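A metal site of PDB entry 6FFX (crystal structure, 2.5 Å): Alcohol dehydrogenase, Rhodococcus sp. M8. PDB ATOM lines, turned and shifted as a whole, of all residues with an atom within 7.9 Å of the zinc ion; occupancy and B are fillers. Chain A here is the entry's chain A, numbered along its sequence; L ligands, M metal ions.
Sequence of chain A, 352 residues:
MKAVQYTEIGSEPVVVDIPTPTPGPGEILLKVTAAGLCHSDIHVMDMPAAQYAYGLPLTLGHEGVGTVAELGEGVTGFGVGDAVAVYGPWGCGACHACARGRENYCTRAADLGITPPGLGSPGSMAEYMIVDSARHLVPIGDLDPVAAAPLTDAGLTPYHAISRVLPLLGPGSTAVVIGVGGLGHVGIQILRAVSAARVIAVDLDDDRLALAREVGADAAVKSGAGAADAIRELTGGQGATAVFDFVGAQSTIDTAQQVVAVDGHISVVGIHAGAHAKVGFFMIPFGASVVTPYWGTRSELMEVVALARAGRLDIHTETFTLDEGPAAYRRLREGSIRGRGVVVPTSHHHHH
CB of Ser 40 touches the zinc ion (3.6 Å).
The side-chain carboxylate (OD2) of Asp 153 is bound to the zinc ion, at 2.0 Å.
NE2 of His 62 is bound to the zinc ion (2.1 Å).
The zinc ion is bound by the side-chain sulfur (SG) of Cys 38 (2.5 Å).
The zinc ion has three donor atoms within binding distance.
The side-chain hydroxyl (OG1) of Thr 157 sits at hydrogen-bond distance from the side-chain carboxylate (OD1) of Asp 153 (2.7 Å).
SG of Cys 38 sits close to NH2 of Arg 340 (3.0 Å).
OD2 of Asp 41 lies within hydrogen-bond range of N of Cys 38 (3.4 Å).
A ring nitrogen (ND1) of His 62 is in hydrogen-bond range of the side-chain carboxylate (OD1) of Asp 41, at 2.9 Å.
SG of Cys 38 sits close to N of Ser 40, at 3.5 Å.
The guanidinium group (NH1) of Arg 340 is in salt-bridge range of an oxygen (O8) of the ligand, at 2.7 Å.
The side-chain hydroxyl (OG) of Ser 40 is in hydrogen-bond range of an oxygen (O13) of the ligand (2.8 Å).
An oxygen (O12) of the ligand lies within hydrogen-bond range of the backbone NH of Ile 271, at 3.4 Å.
An oxygen (O14) of the ligand sits at hydrogen-bond distance from the backbone NH of Trp 295 (3.1 Å).
ND1 of His 39 sits at hydrogen-bond distance from O1 of the ligand (2.9 Å).
The backbone NH of His 39 lies close to an oxygen (O8) of the ligand (3.4 Å).
N of Leu 183 lies within hydrogen-bond range of O9 of the ligand (2.7 Å).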
ATOM      1  N   GLY A  36      -6.387  -3.758  -9.625  1.00  0.00           N
ATOM      2  CA  GLY A  36      -7.611  -3.599  -8.846  1.00  0.00           C
ATOM      3  C   GLY A  36      -7.546  -4.110  -7.401  1.00  0.00           C
ATOM      4  O   GLY A  36      -6.914  -5.127  -7.132  1.00  0.00           O
ATOM      5  N   LEU A  37      -8.200  -3.379  -6.494  1.00  0.00           N
ATOM      6  CA  LEU A  37      -8.364  -3.786  -5.100  1.00  0.00           C
ATOM      7  C   LEU A  37      -9.729  -4.423  -4.944  1.00  0.00           C
ATOM      8  O   LEU A  37     -10.749  -3.789  -5.201  1.00  0.00           O
ATOM      9  CB  LEU A  37      -8.315  -2.590  -4.154  1.00  0.00           C
ATOM     10  CG  LEU A  37      -6.973  -1.921  -3.944  1.00  0.00           C
ATOM     11  CD1 LEU A  37      -6.591  -1.025  -5.116  1.00  0.00           C
ATOM     12  CD2 LEU A  37      -7.004  -1.127  -2.662  1.00  0.00           C
ATOM     13  N   CYS A  38      -9.745  -5.670  -4.488  1.00  0.00           N
ATOM     14  CA  CYS A  38     -10.957  -6.437  -4.289  1.00  0.00           C
ATOM     15  C   CYS A  38     -11.248  -6.638  -2.799  1.00  0.00           C
ATOM     16  O   CYS A  38     -10.320  -6.671  -1.990  1.00  0.00           O
ATOM     17  CB  CYS A  38     -10.857  -7.784  -4.986  1.00  0.00           C
ATOM     18  SG  CYS A  38     -12.411  -8.703  -4.904  1.00  0.00           S
ATOM     19  N   HIS A  39     -12.526  -6.774  -2.453  1.00  0.00           N
ATOM     20  CA  HIS A  39     -12.926  -7.009  -1.057  1.00  0.00           C
ATOM     21  C   HIS A  39     -12.309  -8.328  -0.558  1.00  0.00           C
ATOM     22  O   HIS A  39     -11.988  -8.446   0.614  1.00  0.00           O
ATOM     23  CB  HIS A  39     -14.453  -6.996  -0.894  1.00  0.00           C
ATOM     24  CG  HIS A  39     -14.920  -6.664   0.494  1.00  0.00           C
ATOM     25  ND1 HIS A  39     -15.232  -5.370   0.887  1.00  0.00           N
ATOM     26  CD2 HIS A  39     -15.128  -7.442   1.583  1.00  0.00           C
ATOM     27  CE1 HIS A  39     -15.636  -5.389   2.150  1.00  0.00           C
ATOM     28  NE2 HIS A  39     -15.571  -6.629   2.600  1.00  0.00           N
ATOM     29  N   SER A  40     -12.124  -9.287  -1.460  1.00  0.00           N
ATOM     30  CA  SER A  40     -11.445 -10.534  -1.124  1.00  0.00           C
ATOM     31  C   SER A  40     -10.016 -10.385  -0.583  1.00  0.00           C
ATOM     32  O   SER A  40      -9.572 -11.228   0.187  1.00  0.00           O
ATOM     33  CB  SER A  40     -11.458 -11.506  -2.302  1.00  0.00           C
ATOM     34  OG  SER A  40     -12.787 -11.952  -2.546  1.00  0.00           O
ATOM     35  N   ASP A  41      -9.297  -9.327  -0.981  1.00  0.00           N
ATOM     36  CA  ASP A  41      -7.964  -9.055  -0.436  1.00  0.00           C
ATOM     37  C   ASP A  41      -8.028  -8.746   1.077  1.00  0.00           C
ATOM     38  O   ASP A  41      -7.059  -8.983   1.788  1.00  0.00           O
ATOM     39  CB  ASP A  41      -7.269  -7.902  -1.194  1.00  0.00           C
ATOM     40  CG  ASP A  41      -6.839  -8.265  -2.641  1.00  0.00           C
ATOM     41  OD1 ASP A  41      -6.364  -9.401  -2.892  1.00  0.00           O
ATOM     42  OD2 ASP A  41      -6.938  -7.389  -3.523  1.00  0.00           O
ATOM     43  N   HIS A  62      -5.003  -9.306  -7.314  1.00  0.00           N
ATOM     44  CA  HIS A  62      -5.384 -10.389  -8.231  1.00  0.00           C
ATOM     45  C   HIS A  62      -6.182  -9.915  -9.458  1.00  0.00           C
ATOM     46  O   HIS A  62      -6.458 -10.708 -10.387  1.00  0.00           O
ATOM     47  CB  HIS A  62      -6.086 -11.522  -7.481  1.00  0.00           C
ATOM     48  CG  HIS A  62      -7.276 -11.100  -6.680  1.00  0.00           C
ATOM     49  ND1 HIS A  62      -7.191 -10.680  -5.376  1.00  0.00           N
ATOM     50  CD2 HIS A  62      -8.588 -11.059  -6.999  1.00  0.00           C
ATOM     51  CE1 HIS A  62      -8.404 -10.405  -4.920  1.00  0.00           C
ATOM     52  NE2 HIS A  62      -9.268 -10.620  -5.891  1.00  0.00           N
ATOM     53  N   GLU A  63      -6.518  -8.626  -9.459  1.00  0.00           N
ATOM     54  CA  GLU A  63      -7.062  -7.944 -10.618  1.00  0.00           C
ATOM     55  C   GLU A  63      -5.941  -7.182 -11.310  1.00  0.00           C
ATOM     56  O   GLU A  63      -5.555  -6.118 -10.855  1.00  0.00           O
ATOM     57  CB  GLU A  63      -8.166  -6.945 -10.206  1.00  0.00           C
ATOM     58  CG  GLU A  63      -9.490  -7.551  -9.788  1.00  0.00           C
ATOM     59  CD  GLU A  63     -10.569  -6.522  -9.549  1.00  0.00           C
ATOM     60  OE1 GLU A  63     -10.273  -5.360  -9.192  1.00  0.00           O
ATOM     61  OE2 GLU A  63     -11.753  -6.870  -9.688  1.00  0.00           O
ATOM     62  N   LEU A 119      -2.875 -14.182  -4.547  1.00  0.00           N
ATOM     63  CA  LEU A 119      -3.444 -15.153  -3.611  1.00  0.00           C
ATOM     64  C   LEU A 119      -2.552 -16.399  -3.588  1.00  0.00           C
ATOM     65  O   LEU A 119      -3.046 -17.519  -3.655  1.00  0.00           O
ATOM     66  CB  LEU A 119      -4.889 -15.519  -4.031  1.00  0.00           C
ATOM     67  CG  LEU A 119      -5.901 -14.392  -4.286  1.00  0.00           C
ATOM     68  CD1 LEU A 119      -7.143 -14.942  -4.974  1.00  0.00           C
ATOM     69  CD2 LEU A 119      -6.306 -13.688  -3.016  1.00  0.00           C
ATOM     70  N   THR A 152     -11.318  -8.160 -14.643  1.00  0.00           N
ATOM     71  CA  THR A 152     -10.699  -9.459 -14.351  1.00  0.00           C
ATOM     72  C   THR A 152     -11.302 -10.223 -13.163  1.00  0.00           C
ATOM     73  O   THR A 152     -11.039 -11.424 -13.005  1.00  0.00           O
ATOM     74  CB  THR A 152      -9.190  -9.303 -14.068  1.00  0.00           C
ATOM     75  OG1 THR A 152      -8.966  -8.473 -12.923  1.00  0.00           O
ATOM     76  CG2 THR A 152      -8.478  -8.711 -15.267  1.00  0.00           C
ATOM     77  N   ASP A 153     -12.069  -9.517 -12.337  1.00  0.00           N
ATOM     78  CA  ASP A 153     -12.718 -10.132 -11.192  1.00  0.00           C
ATOM     79  C   ASP A 153     -14.106  -9.521 -10.922  1.00  0.00           C
ATOM     80  O   ASP A 153     -15.123 -10.243 -10.929  1.00  0.00           O
ATOM     81  CB  ASP A 153     -11.820  -9.976  -9.966  1.00  0.00           C
ATOM     82  CG  ASP A 153     -12.284 -10.779  -8.776  1.00  0.00           C
ATOM     83  OD1 ASP A 153     -13.270 -11.546  -8.851  1.00  0.00           O
ATOM     84  OD2 ASP A 153     -11.626 -10.593  -7.738  1.00  0.00           O
ATOM     85  N   ALA A 154     -14.148  -8.199 -10.700  1.00  0.00           N
ATOM     86  CA  ALA A 154     -15.399  -7.493 -10.499  1.00  0.00           C
ATOM     87  C   ALA A 154     -16.373  -7.648 -11.675  1.00  0.00           C
ATOM     88  O   ALA A 154     -17.571  -7.642 -11.456  1.00  0.00           O
ATOM     89  CB  ALA A 154     -15.144  -6.029 -10.226  1.00  0.00           C
ATOM     90  N   THR A 157     -16.451 -12.249 -12.211  1.00  0.00           N
ATOM     91  CA  THR A 157     -17.153 -13.052 -11.210  1.00  0.00           C
ATOM     92  C   THR A 157     -18.691 -12.956 -11.353  1.00  0.00           C
ATOM     93  O   THR A 157     -19.350 -13.991 -11.382  1.00  0.00           O
ATOM     94  CB  THR A 157     -16.701 -12.728  -9.792  1.00  0.00           C
ATOM     95  OG1 THR A 157     -15.331 -13.078  -9.653  1.00  0.00           O
ATOM     96  CG2 THR A 157     -17.505 -13.460  -8.771  1.00  0.00           C
ATOM     97  N   LEU A 183     -18.681  -5.472  -7.391  1.00  0.00           N
ATOM     98  CA  LEU A 183     -19.211  -6.531  -8.219  1.00  0.00           C
ATOM     99  C   LEU A 183     -20.612  -6.237  -8.735  1.00  0.00           C
ATOM    100  O   LEU A 183     -20.909  -6.356  -9.945  1.00  0.00           O
ATOM    101  CB  LEU A 183     -19.204  -7.869  -7.476  1.00  0.00           C
ATOM    102  CG  LEU A 183     -17.959  -8.738  -7.622  1.00  0.00           C
ATOM    103  CD1 LEU A 183     -16.738  -8.065  -7.054  1.00  0.00           C
ATOM    104  CD2 LEU A 183     -18.137 -10.068  -6.936  1.00  0.00           C
ATOM    105  N   ILE A 271     -19.167 -13.515   0.262  1.00  0.00           N
ATOM    106  CA  ILE A 271     -18.567 -14.464   1.192  1.00  0.00           C
ATOM    107  C   ILE A 271     -18.665 -13.933   2.618  1.00  0.00           C
ATOM    108  O   ILE A 271     -18.027 -12.974   2.963  1.00  0.00           O
ATOM    109  CB  ILE A 271     -17.087 -14.700   0.796  1.00  0.00           C
ATOM    110  CG1 ILE A 271     -17.016 -15.304  -0.611  1.00  0.00           C
ATOM    111  CG2 ILE A 271     -16.385 -15.584   1.814  1.00  0.00           C
ATOM    112  CD1 ILE A 271     -15.641 -15.420  -1.214  1.00  0.00           C
ATOM    113  N   TRP A 295     -15.218 -17.149  -9.140  1.00  0.00           N
ATOM    114  CA  TRP A 295     -14.492 -16.434 -10.156  1.00  0.00           C
ATOM    115  C   TRP A 295     -15.130 -16.693 -11.533  1.00  0.00           C
ATOM    116  O   TRP A 295     -16.325 -16.542 -11.644  1.00  0.00           O
ATOM    117  CB  TRP A 295     -12.994 -16.762 -10.056  1.00  0.00           C
ATOM    118  CG  TRP A 295     -12.089 -15.595 -10.304  1.00  0.00           C
ATOM    119  CD1 TRP A 295     -12.320 -14.521 -11.134  1.00  0.00           C
ATOM    120  CD2 TRP A 295     -10.793 -15.377  -9.734  1.00  0.00           C
ATOM    121  NE1 TRP A 295     -11.253 -13.655 -11.103  1.00  0.00           N
ATOM    122  CE2 TRP A 295     -10.302 -14.161 -10.245  1.00  0.00           C
ATOM    123  CE3 TRP A 295      -9.994 -16.088  -8.831  1.00  0.00           C
ATOM    124  CZ2 TRP A 295      -9.050 -13.646  -9.889  1.00  0.00           C
ATOM    125  CZ3 TRP A 295      -8.748 -15.573  -8.483  1.00  0.00           C
ATOM    126  CH2 TRP A 295      -8.298 -14.370  -9.003  1.00  0.00           C
ATOM    127  N   ARG A 340     -15.010   0.563  -7.656  1.00  0.00           N
ATOM    128  CA  ARG A 340     -13.784  -0.220  -7.513  1.00  0.00           C
ATOM    129  C   ARG A 340     -12.551   0.666  -7.412  1.00  0.00           C
ATOM    130  O   ARG A 340     -12.400   1.626  -8.162  1.00  0.00           O
ATOM    131  CB  ARG A 340     -13.638  -1.159  -8.702  1.00  0.00           C
ATOM    132  CG  ARG A 340     -12.656  -2.298  -8.439  1.00  0.00           C
ATOM    133  CD  ARG A 340     -13.104  -3.168  -7.308  1.00  0.00           C
ATOM    134  NE  ARG A 340     -12.838  -4.605  -7.487  1.00  0.00           N
ATOM    135  CZ  ARG A 340     -13.524  -5.569  -6.883  1.00  0.00           C
ATOM    136  NH1 ARG A 340     -14.503  -5.304  -6.029  1.00  0.00           N
ATOM    137  NH2 ARG A 340     -13.205  -6.840  -7.100  1.00  0.00           N
HETATM  138  P1  LIG L   1     -17.640  -3.930  -2.096  1.00  0.00           P
HETATM  139  O1  LIG L   1     -17.028  -3.733  -0.713  1.00  0.00           O
HETATM  140  O2  LIG L   1     -17.000  -3.313  -3.307  1.00  0.00           O
HETATM  141  O3  LIG L   1     -19.188  -3.502  -2.055  1.00  0.00           O
HETATM  142  C1  LIG L   1     -20.071  -3.978  -1.055  1.00  0.00           C
HETATM  143  C2  LIG L   1     -21.499  -3.497  -1.313  1.00  0.00           C
HETATM  144  O4  LIG L   1     -22.384  -4.362  -0.610  1.00  0.00           O
HETATM  145  C3  LIG L   1     -21.761  -2.084  -0.809  1.00  0.00           C
HETATM  146  O5  LIG L   1     -22.513  -1.337  -1.780  1.00  0.00           O
HETATM  147  C4  LIG L   1     -22.541  -2.274   0.480  1.00  0.00           C
HETATM  148  O6  LIG L   1     -23.418  -1.183   0.811  1.00  0.00           O
HETATM  149  C5  LIG L   1     -23.288  -3.575   0.188  1.00  0.00           C
HETATM  150  N1  LIG L   1     -23.817  -4.264   1.408  1.00  0.00           N
HETATM  151  C6  LIG L   1     -23.175  -4.527   2.582  1.00  0.00           C
HETATM  152  N2  LIG L   1     -24.016  -5.155   3.459  1.00  0.00           N
HETATM  153  C7  LIG L   1     -25.213  -5.292   2.833  1.00  0.00           C
HETATM  154  C8  LIG L   1     -26.558  -5.854   3.156  1.00  0.00           C
HETATM  155  N3  LIG L   1     -26.817  -6.410   4.349  1.00  0.00           N
HETATM  156  N4  LIG L   1     -27.536  -5.799   2.223  1.00  0.00           N
HETATM  157  C9  LIG L   1     -27.322  -5.245   0.999  1.00  0.00           C
HETATM  158  N5  LIG L   1     -26.140  -4.704   0.629  1.00  0.00           N
HETATM  159  C10 LIG L   1     -25.078  -4.698   1.481  1.00  0.00           C
HETATM  160  O7  LIG L   1     -17.784  -5.505  -2.384  1.00  0.00           O
HETATM  161  P2  LIG L   1     -17.111  -6.290  -3.629  1.00  0.00           P
HETATM  162  O8  LIG L   1     -15.628  -6.019  -3.705  1.00  0.00           O
HETATM  163  O9  LIG L   1     -18.042  -6.060  -4.788  1.00  0.00           O
HETATM  164  O10 LIG L   1     -17.278  -7.838  -3.213  1.00  0.00           O
HETATM  165  C11 LIG L   1     -18.466  -8.293  -2.551  1.00  0.00           C
HETATM  166  C12 LIG L   1     -18.256  -9.723  -2.077  1.00  0.00           C
HETATM  167  O11 LIG L   1     -17.934 -10.551  -3.205  1.00  0.00           O
HETATM  168  C13 LIG L   1     -17.117  -9.840  -1.060  1.00  0.00           C
HETATM  169  O12 LIG L   1     -17.565 -10.570   0.095  1.00  0.00           O
HETATM  170  C14 LIG L   1     -16.004 -10.530  -1.855  1.00  0.00           C
HETATM  171  O13 LIG L   1     -15.099 -11.288  -1.036  1.00  0.00           O
HETATM  172  C15 LIG L   1     -16.821 -11.383  -2.841  1.00  0.00           C
HETATM  173  N6  LIG L   1     -16.139 -11.878  -4.046  1.00  0.00           N
HETATM  174  C16 LIG L   1     -16.312 -13.171  -4.401  1.00  0.00           C
HETATM  175  C17 LIG L   1     -15.701 -13.725  -5.522  1.00  0.00           C
HETATM  176  C18 LIG L   1     -15.918 -15.182  -5.882  1.00  0.00           C
HETATM  177  O14 LIG L   1     -14.988 -15.790  -6.361  1.00  0.00           O
HETATM  178  N7  LIG L   1     -17.117 -15.776  -5.706  1.00  0.00           N
HETATM  179  C19 LIG L   1     -14.882 -12.912  -6.313  1.00  0.00           C
HETATM  180  C20 LIG L   1     -14.733 -11.570  -5.966  1.00  0.00           C
HETATM  181  C21 LIG L   1     -15.367 -11.069  -4.816  1.00  0.00           C
HETATM  182 ZN    ZN M   1     -11.410 -10.764  -5.782  1.00  0.00          ZN
